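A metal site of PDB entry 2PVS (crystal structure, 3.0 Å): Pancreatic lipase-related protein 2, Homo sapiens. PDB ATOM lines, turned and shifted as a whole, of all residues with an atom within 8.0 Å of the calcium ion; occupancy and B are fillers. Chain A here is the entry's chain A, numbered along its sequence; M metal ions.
O of Glu 189 binds the calcium ion (2.2 Å).
OD2 of Asp 194 binds the calcium ion (2.3 Å).
O of Arg 192 is bound to the calcium ion, at 2.4 Å.
The side-chain carboxylate (OD1) of Asp 197 binds the calcium ion.
OD2 of Asp 197 is bound to the calcium ion, 2.7 Å away.
The calcium ion has five donor atoms within binding distance.
The side-chain hydroxyl (OG) of Ser 196 sits close to the side-chain carboxylate (OD1) of Asp 194, at 3.0 Å.
OD1 of Asp 197 sits close to OG of Ser 196, 3.2 Å away.
Within 4 Å of the calcium ion: Glu 189, Arg 192, Asp 194 and Asp 197.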
ATOM      1  N   TRP A  17     -34.367  11.711   2.500  1.00  0.00           N
ATOM      2  CA  TRP A  17     -33.014  12.241   2.651  1.00  0.00           C
ATOM      3  C   TRP A  17     -32.562  12.342   4.101  1.00  0.00           C
ATOM      4  O   TRP A  17     -31.384  12.134   4.378  1.00  0.00           O
ATOM      5  CB  TRP A  17     -32.914  13.627   2.010  1.00  0.00           C
ATOM      6  CG  TRP A  17     -33.102  13.563   0.557  1.00  0.00           C
ATOM      7  CD1 TRP A  17     -34.207  13.915  -0.140  1.00  0.00           C
ATOM      8  CD2 TRP A  17     -32.166  13.057  -0.400  1.00  0.00           C
ATOM      9  NE1 TRP A  17     -34.016  13.686  -1.469  1.00  0.00           N
ATOM     10  CE2 TRP A  17     -32.771  13.155  -1.660  1.00  0.00           C
ATOM     11  CE3 TRP A  17     -30.884  12.541  -0.318  1.00  0.00           C
ATOM     12  CZ2 TRP A  17     -32.130  12.761  -2.833  1.00  0.00           C
ATOM     13  CZ3 TRP A  17     -30.249  12.148  -1.484  1.00  0.00           C
ATOM     14  CH2 TRP A  17     -30.869  12.260  -2.719  1.00  0.00           C
ATOM     15  N   HIS A 158     -22.144   5.965  -3.841  1.00  0.00           N
ATOM     16  CA  HIS A 158     -23.421   6.659  -3.809  1.00  0.00           C
ATOM     17  C   HIS A 158     -23.309   8.074  -4.382  1.00  0.00           C
ATOM     18  O   HIS A 158     -24.281   8.601  -4.903  1.00  0.00           O
ATOM     19  CB  HIS A 158     -23.961   6.678  -2.384  1.00  0.00           C
ATOM     20  CG  HIS A 158     -24.159   5.318  -1.813  1.00  0.00           C
ATOM     21  ND1 HIS A 158     -25.003   4.394  -2.390  1.00  0.00           N
ATOM     22  CD2 HIS A 158     -23.605   4.702  -0.743  1.00  0.00           C
ATOM     23  CE1 HIS A 158     -24.966   3.271  -1.689  1.00  0.00           C
ATOM     24  NE2 HIS A 158     -24.127   3.429  -0.691  1.00  0.00           N
ATOM     25  N   ALA A 160     -21.276   8.790  -7.002  1.00  0.00           N
ATOM     26  CA  ALA A 160     -21.467   8.440  -8.406  1.00  0.00           C
ATOM     27  C   ALA A 160     -22.949   8.314  -8.694  1.00  0.00           C
ATOM     28  O   ALA A 160     -23.430   8.886  -9.646  1.00  0.00           O
ATOM     29  CB  ALA A 160     -20.778   7.127  -8.725  1.00  0.00           C
ATOM     30  N   ALA A 161     -23.664   7.587  -7.838  1.00  0.00           N
ATOM     31  CA  ALA A 161     -25.066   7.243  -8.100  1.00  0.00           C
ATOM     32  C   ALA A 161     -25.958   8.461  -8.105  1.00  0.00           C
ATOM     33  O   ALA A 161     -27.055   8.462  -8.706  1.00  0.00           O
ATOM     34  CB  ALA A 161     -25.562   6.256  -7.074  1.00  0.00           C
ATOM     35  N   GLU A 162     -25.498   9.501  -7.415  1.00  0.00           N
ATOM     36  CA  GLU A 162     -26.243  10.755  -7.309  1.00  0.00           C
ATOM     37  C   GLU A 162     -26.082  11.518  -8.600  1.00  0.00           C
ATOM     38  O   GLU A 162     -27.060  11.967  -9.175  1.00  0.00           O
ATOM     39  CB  GLU A 162     -25.711  11.576  -6.148  1.00  0.00           C
ATOM     40  CG  GLU A 162     -26.269  12.987  -6.065  1.00  0.00           C
ATOM     41  CD  GLU A 162     -27.741  13.016  -5.729  1.00  0.00           C
ATOM     42  OE1 GLU A 162     -28.332  14.126  -5.732  1.00  0.00           O
ATOM     43  OE2 GLU A 162     -28.321  11.920  -5.446  1.00  0.00           O
ATOM     44  N   GLY A 164     -25.194  10.221 -11.422  1.00  0.00           N
ATOM     45  CA  GLY A 164     -25.834   9.417 -12.467  1.00  0.00           C
ATOM     46  C   GLY A 164     -27.319   9.693 -12.587  1.00  0.00           C
ATOM     47  O   GLY A 164     -27.850   9.795 -13.686  1.00  0.00           O
ATOM     48  N   ARG A 165     -27.968   9.790 -11.430  1.00  0.00           N
ATOM     49  CA  ARG A 165     -29.382  10.089 -11.357  1.00  0.00           C
ATOM     50  C   ARG A 165     -29.696  11.525 -11.793  1.00  0.00           C
ATOM     51  O   ARG A 165     -30.709  11.752 -12.472  1.00  0.00           O
ATOM     52  CB  ARG A 165     -29.871   9.903  -9.930  1.00  0.00           C
ATOM     53  CG  ARG A 165     -31.373   9.990  -9.784  1.00  0.00           C
ATOM     54  CD  ARG A 165     -31.784  10.136  -8.319  1.00  0.00           C
ATOM     55  NE  ARG A 165     -31.106  11.271  -7.692  1.00  0.00           N
ATOM     56  CZ  ARG A 165     -31.681  12.358  -7.227  1.00  0.00           C
ATOM     57  NH1 ARG A 165     -30.942  13.318  -6.688  1.00  0.00           N
ATOM     58  NH2 ARG A 165     -32.999  12.527  -7.273  1.00  0.00           N
ATOM     59  N   ARG A 166     -28.856  12.475 -11.405  1.00  0.00           N
ATOM     60  CA  ARG A 166     -28.907  13.853 -11.944  1.00  0.00           C
ATOM     61  C   ARG A 166     -28.913  13.866 -13.461  1.00  0.00           C
ATOM     62  O   ARG A 166     -29.585  14.684 -14.056  1.00  0.00           O
ATOM     63  CB  ARG A 166     -27.702  14.683 -11.489  1.00  0.00           C
ATOM     64  CG  ARG A 166     -27.982  15.757 -10.477  1.00  0.00           C
ATOM     65  CD  ARG A 166     -28.695  15.214  -9.292  1.00  0.00           C
ATOM     66  NE  ARG A 166     -28.323  15.893  -8.051  1.00  0.00           N
ATOM     67  CZ  ARG A 166     -28.593  17.174  -7.753  1.00  0.00           C
ATOM     68  NH1 ARG A 166     -28.216  17.642  -6.573  1.00  0.00           N
ATOM     69  NH2 ARG A 166     -29.202  18.000  -8.609  1.00  0.00           N
ATOM     70  N   ILE A 174     -21.526   3.201 -14.208  1.00  0.00           N
ATOM     71  CA  ILE A 174     -21.089   3.448 -12.835  1.00  0.00           C
ATOM     72  C   ILE A 174     -20.508   2.141 -12.288  1.00  0.00           C
ATOM     73  O   ILE A 174     -21.080   1.065 -12.518  1.00  0.00           O
ATOM     74  CB  ILE A 174     -22.216   4.024 -11.928  1.00  0.00           C
ATOM     75  CG1 ILE A 174     -22.633   5.414 -12.451  1.00  0.00           C
ATOM     76  CG2 ILE A 174     -21.755   4.133 -10.484  1.00  0.00           C
ATOM     77  CD1 ILE A 174     -23.739   6.150 -11.671  1.00  0.00           C
ATOM     78  N   PRO A 188     -34.587   3.870  -0.163  1.00  0.00           N
ATOM     79  CA  PRO A 188     -35.158   4.110  -1.461  1.00  0.00           C
ATOM     80  C   PRO A 188     -34.122   4.402  -2.525  1.00  0.00           C
ATOM     81  O   PRO A 188     -33.123   5.064  -2.240  1.00  0.00           O
ATOM     82  CB  PRO A 188     -36.001   5.365  -1.227  1.00  0.00           C
ATOM     83  CG  PRO A 188     -36.307   5.349   0.172  1.00  0.00           C
ATOM     84  CD  PRO A 188     -35.069   4.866   0.805  1.00  0.00           C
ATOM     85  N   GLU A 189     -34.401   3.988  -3.753  1.00  0.00           N
ATOM     86  CA  GLU A 189     -33.459   4.127  -4.863  1.00  0.00           C
ATOM     87  C   GLU A 189     -32.901   5.550  -5.095  1.00  0.00           C
ATOM     88  O   GLU A 189     -31.799   5.693  -5.627  1.00  0.00           O
ATOM     89  CB  GLU A 189     -34.098   3.625  -6.155  1.00  0.00           C
ATOM     90  CG  GLU A 189     -34.487   2.157  -6.090  1.00  0.00           C
ATOM     91  CD  GLU A 189     -34.959   1.605  -7.422  1.00  0.00           C
ATOM     92  OE1 GLU A 189     -36.065   1.981  -7.879  1.00  0.00           O
ATOM     93  OE2 GLU A 189     -34.218   0.771  -8.008  1.00  0.00           O
ATOM     94  N   GLU A 190     -33.653   6.576  -4.708  1.00  0.00           N
ATOM     95  CA  GLU A 190     -33.275   7.949  -5.009  1.00  0.00           C
ATOM     96  C   GLU A 190     -32.001   8.345  -4.251  1.00  0.00           C
ATOM     97  O   GLU A 190     -31.159   9.117  -4.757  1.00  0.00           O
ATOM     98  CB  GLU A 190     -34.440   8.925  -4.733  1.00  0.00           C
ATOM     99  CG  GLU A 190     -34.678   9.980  -5.891  1.00  0.00           C
ATOM    100  CD  GLU A 190     -35.669   9.538  -7.074  1.00  0.00           C
ATOM    101  OE1 GLU A 190     -35.445   8.500  -7.776  1.00  0.00           O
ATOM    102  OE2 GLU A 190     -36.662  10.285  -7.317  1.00  0.00           O
ATOM    103  N   VAL A 191     -31.852   7.765  -3.058  1.00  0.00           N
ATOM    104  CA  VAL A 191     -30.785   8.166  -2.130  1.00  0.00           C
ATOM    105  C   VAL A 191     -29.542   7.274  -2.204  1.00  0.00           C
ATOM    106  O   VAL A 191     -28.609   7.466  -1.420  1.00  0.00           O
ATOM    107  CB  VAL A 191     -31.314   8.189  -0.683  1.00  0.00           C
ATOM    108  CG1 VAL A 191     -32.471   9.170  -0.558  1.00  0.00           C
ATOM    109  CG2 VAL A 191     -31.734   6.780  -0.228  1.00  0.00           C
ATOM    110  N   ARG A 192     -29.517   6.347  -3.149  1.00  0.00           N
ATOM    111  CA  ARG A 192     -28.445   5.351  -3.235  1.00  0.00           C
ATOM    112  C   ARG A 192     -28.203   4.796  -4.631  1.00  0.00           C
ATOM    113  O   ARG A 192     -28.987   4.994  -5.536  1.00  0.00           O
ATOM    114  CB  ARG A 192     -28.803   4.184  -2.324  1.00  0.00           C
ATOM    115  CG  ARG A 192     -30.000   3.394  -2.781  1.00  0.00           C
ATOM    116  CD  ARG A 192     -29.898   1.999  -2.262  1.00  0.00           C
ATOM    117  NE  ARG A 192     -31.176   1.299  -2.335  1.00  0.00           N
ATOM    118  CZ  ARG A 192     -31.556   0.529  -3.346  1.00  0.00           C
ATOM    119  NH1 ARG A 192     -32.748  -0.050  -3.270  1.00  0.00           N
ATOM    120  NH2 ARG A 192     -30.784   0.329  -4.412  1.00  0.00           N
ATOM    121  N   LEU A 193     -27.121   4.043  -4.782  1.00  0.00           N
ATOM    122  CA  LEU A 193     -26.800   3.397  -6.046  1.00  0.00           C
ATOM    123  C   LEU A 193     -27.798   2.303  -6.353  1.00  0.00           C
ATOM    124  O   LEU A 193     -28.208   1.572  -5.473  1.00  0.00           O
ATOM    125  CB  LEU A 193     -25.396   2.797  -6.021  1.00  0.00           C
ATOM    126  CG  LEU A 193     -24.913   2.212  -7.335  1.00  0.00           C
ATOM    127  CD1 LEU A 193     -24.903   3.308  -8.394  1.00  0.00           C
ATOM    128  CD2 LEU A 193     -23.544   1.553  -7.159  1.00  0.00           C
ATOM    129  N   ASP A 194     -28.178   2.215  -7.619  1.00  0.00           N
ATOM    130  CA  ASP A 194     -29.116   1.202  -8.061  1.00  0.00           C
ATOM    131  C   ASP A 194     -29.059   1.157  -9.569  1.00  0.00           C
ATOM    132  O   ASP A 194     -28.698   2.146 -10.200  1.00  0.00           O
ATOM    133  CB  ASP A 194     -30.544   1.513  -7.614  1.00  0.00           C
ATOM    134  CG  ASP A 194     -31.155   2.686  -8.380  1.00  0.00           C
ATOM    135  OD1 ASP A 194     -32.006   2.399  -9.261  1.00  0.00           O
ATOM    136  OD2 ASP A 194     -30.768   3.863  -8.109  1.00  0.00           O
ATOM    137  N   PRO A 195     -29.435   0.029 -10.163  1.00  0.00           N
ATOM    138  CA  PRO A 195     -29.142  -0.143 -11.575  1.00  0.00           C
ATOM    139  C   PRO A 195     -29.710   0.965 -12.476  1.00  0.00           C
ATOM    140  O   PRO A 195     -29.230   1.138 -13.610  1.00  0.00           O
ATOM    141  CB  PRO A 195     -29.783  -1.494 -11.900  1.00  0.00           C
ATOM    142  CG  PRO A 195     -29.828  -2.197 -10.593  1.00  0.00           C
ATOM    143  CD  PRO A 195     -30.123  -1.136  -9.604  1.00  0.00           C
ATOM    144  N   SER A 196     -30.698   1.712 -11.966  1.00  0.00           N
ATOM    145  CA  SER A 196     -31.287   2.819 -12.715  1.00  0.00           C
ATOM    146  C   SER A 196     -30.293   3.927 -13.007  1.00  0.00           C
ATOM    147  O   SER A 196     -30.503   4.681 -13.933  1.00  0.00           O
ATOM    148  CB  SER A 196     -32.452   3.440 -11.949  1.00  0.00           C
ATOM    149  OG  SER A 196     -32.030   4.605 -11.274  1.00  0.00           O
ATOM    150  N   ASP A 197     -29.219   4.054 -12.243  1.00  0.00           N
ATOM    151  CA  ASP A 197     -28.417   5.287 -12.246  1.00  0.00           C
ATOM    152  C   ASP A 197     -27.422   5.424 -13.417  1.00  0.00           C
ATOM    153  O   ASP A 197     -26.803   6.470 -13.596  1.00  0.00           O
ATOM    154  CB  ASP A 197     -27.696   5.447 -10.903  1.00  0.00           C
ATOM    155  CG  ASP A 197     -28.663   5.458  -9.712  1.00  0.00           C
ATOM    156  OD1 ASP A 197     -29.663   6.228  -9.771  1.00  0.00           O
ATOM    157  OD2 ASP A 197     -28.455   4.719  -8.726  1.00  0.00           O
ATOM    158  N   ALA A 198     -27.268   4.374 -14.224  1.00  0.00           N
ATOM    159  CA  ALA A 198     -26.407   4.424 -15.407  1.00  0.00           C
ATOM    160  C   ALA A 198     -26.849   3.361 -16.387  1.00  0.00           C
ATOM    161  O   ALA A 198     -27.639   2.461 -16.062  1.00  0.00           O
ATOM    162  CB  ALA A 198     -24.954   4.225 -15.029  1.00  0.00           C
HETATM  163 CA    CA M   1     -30.296   5.972  -7.272  1.00  0.00          CA
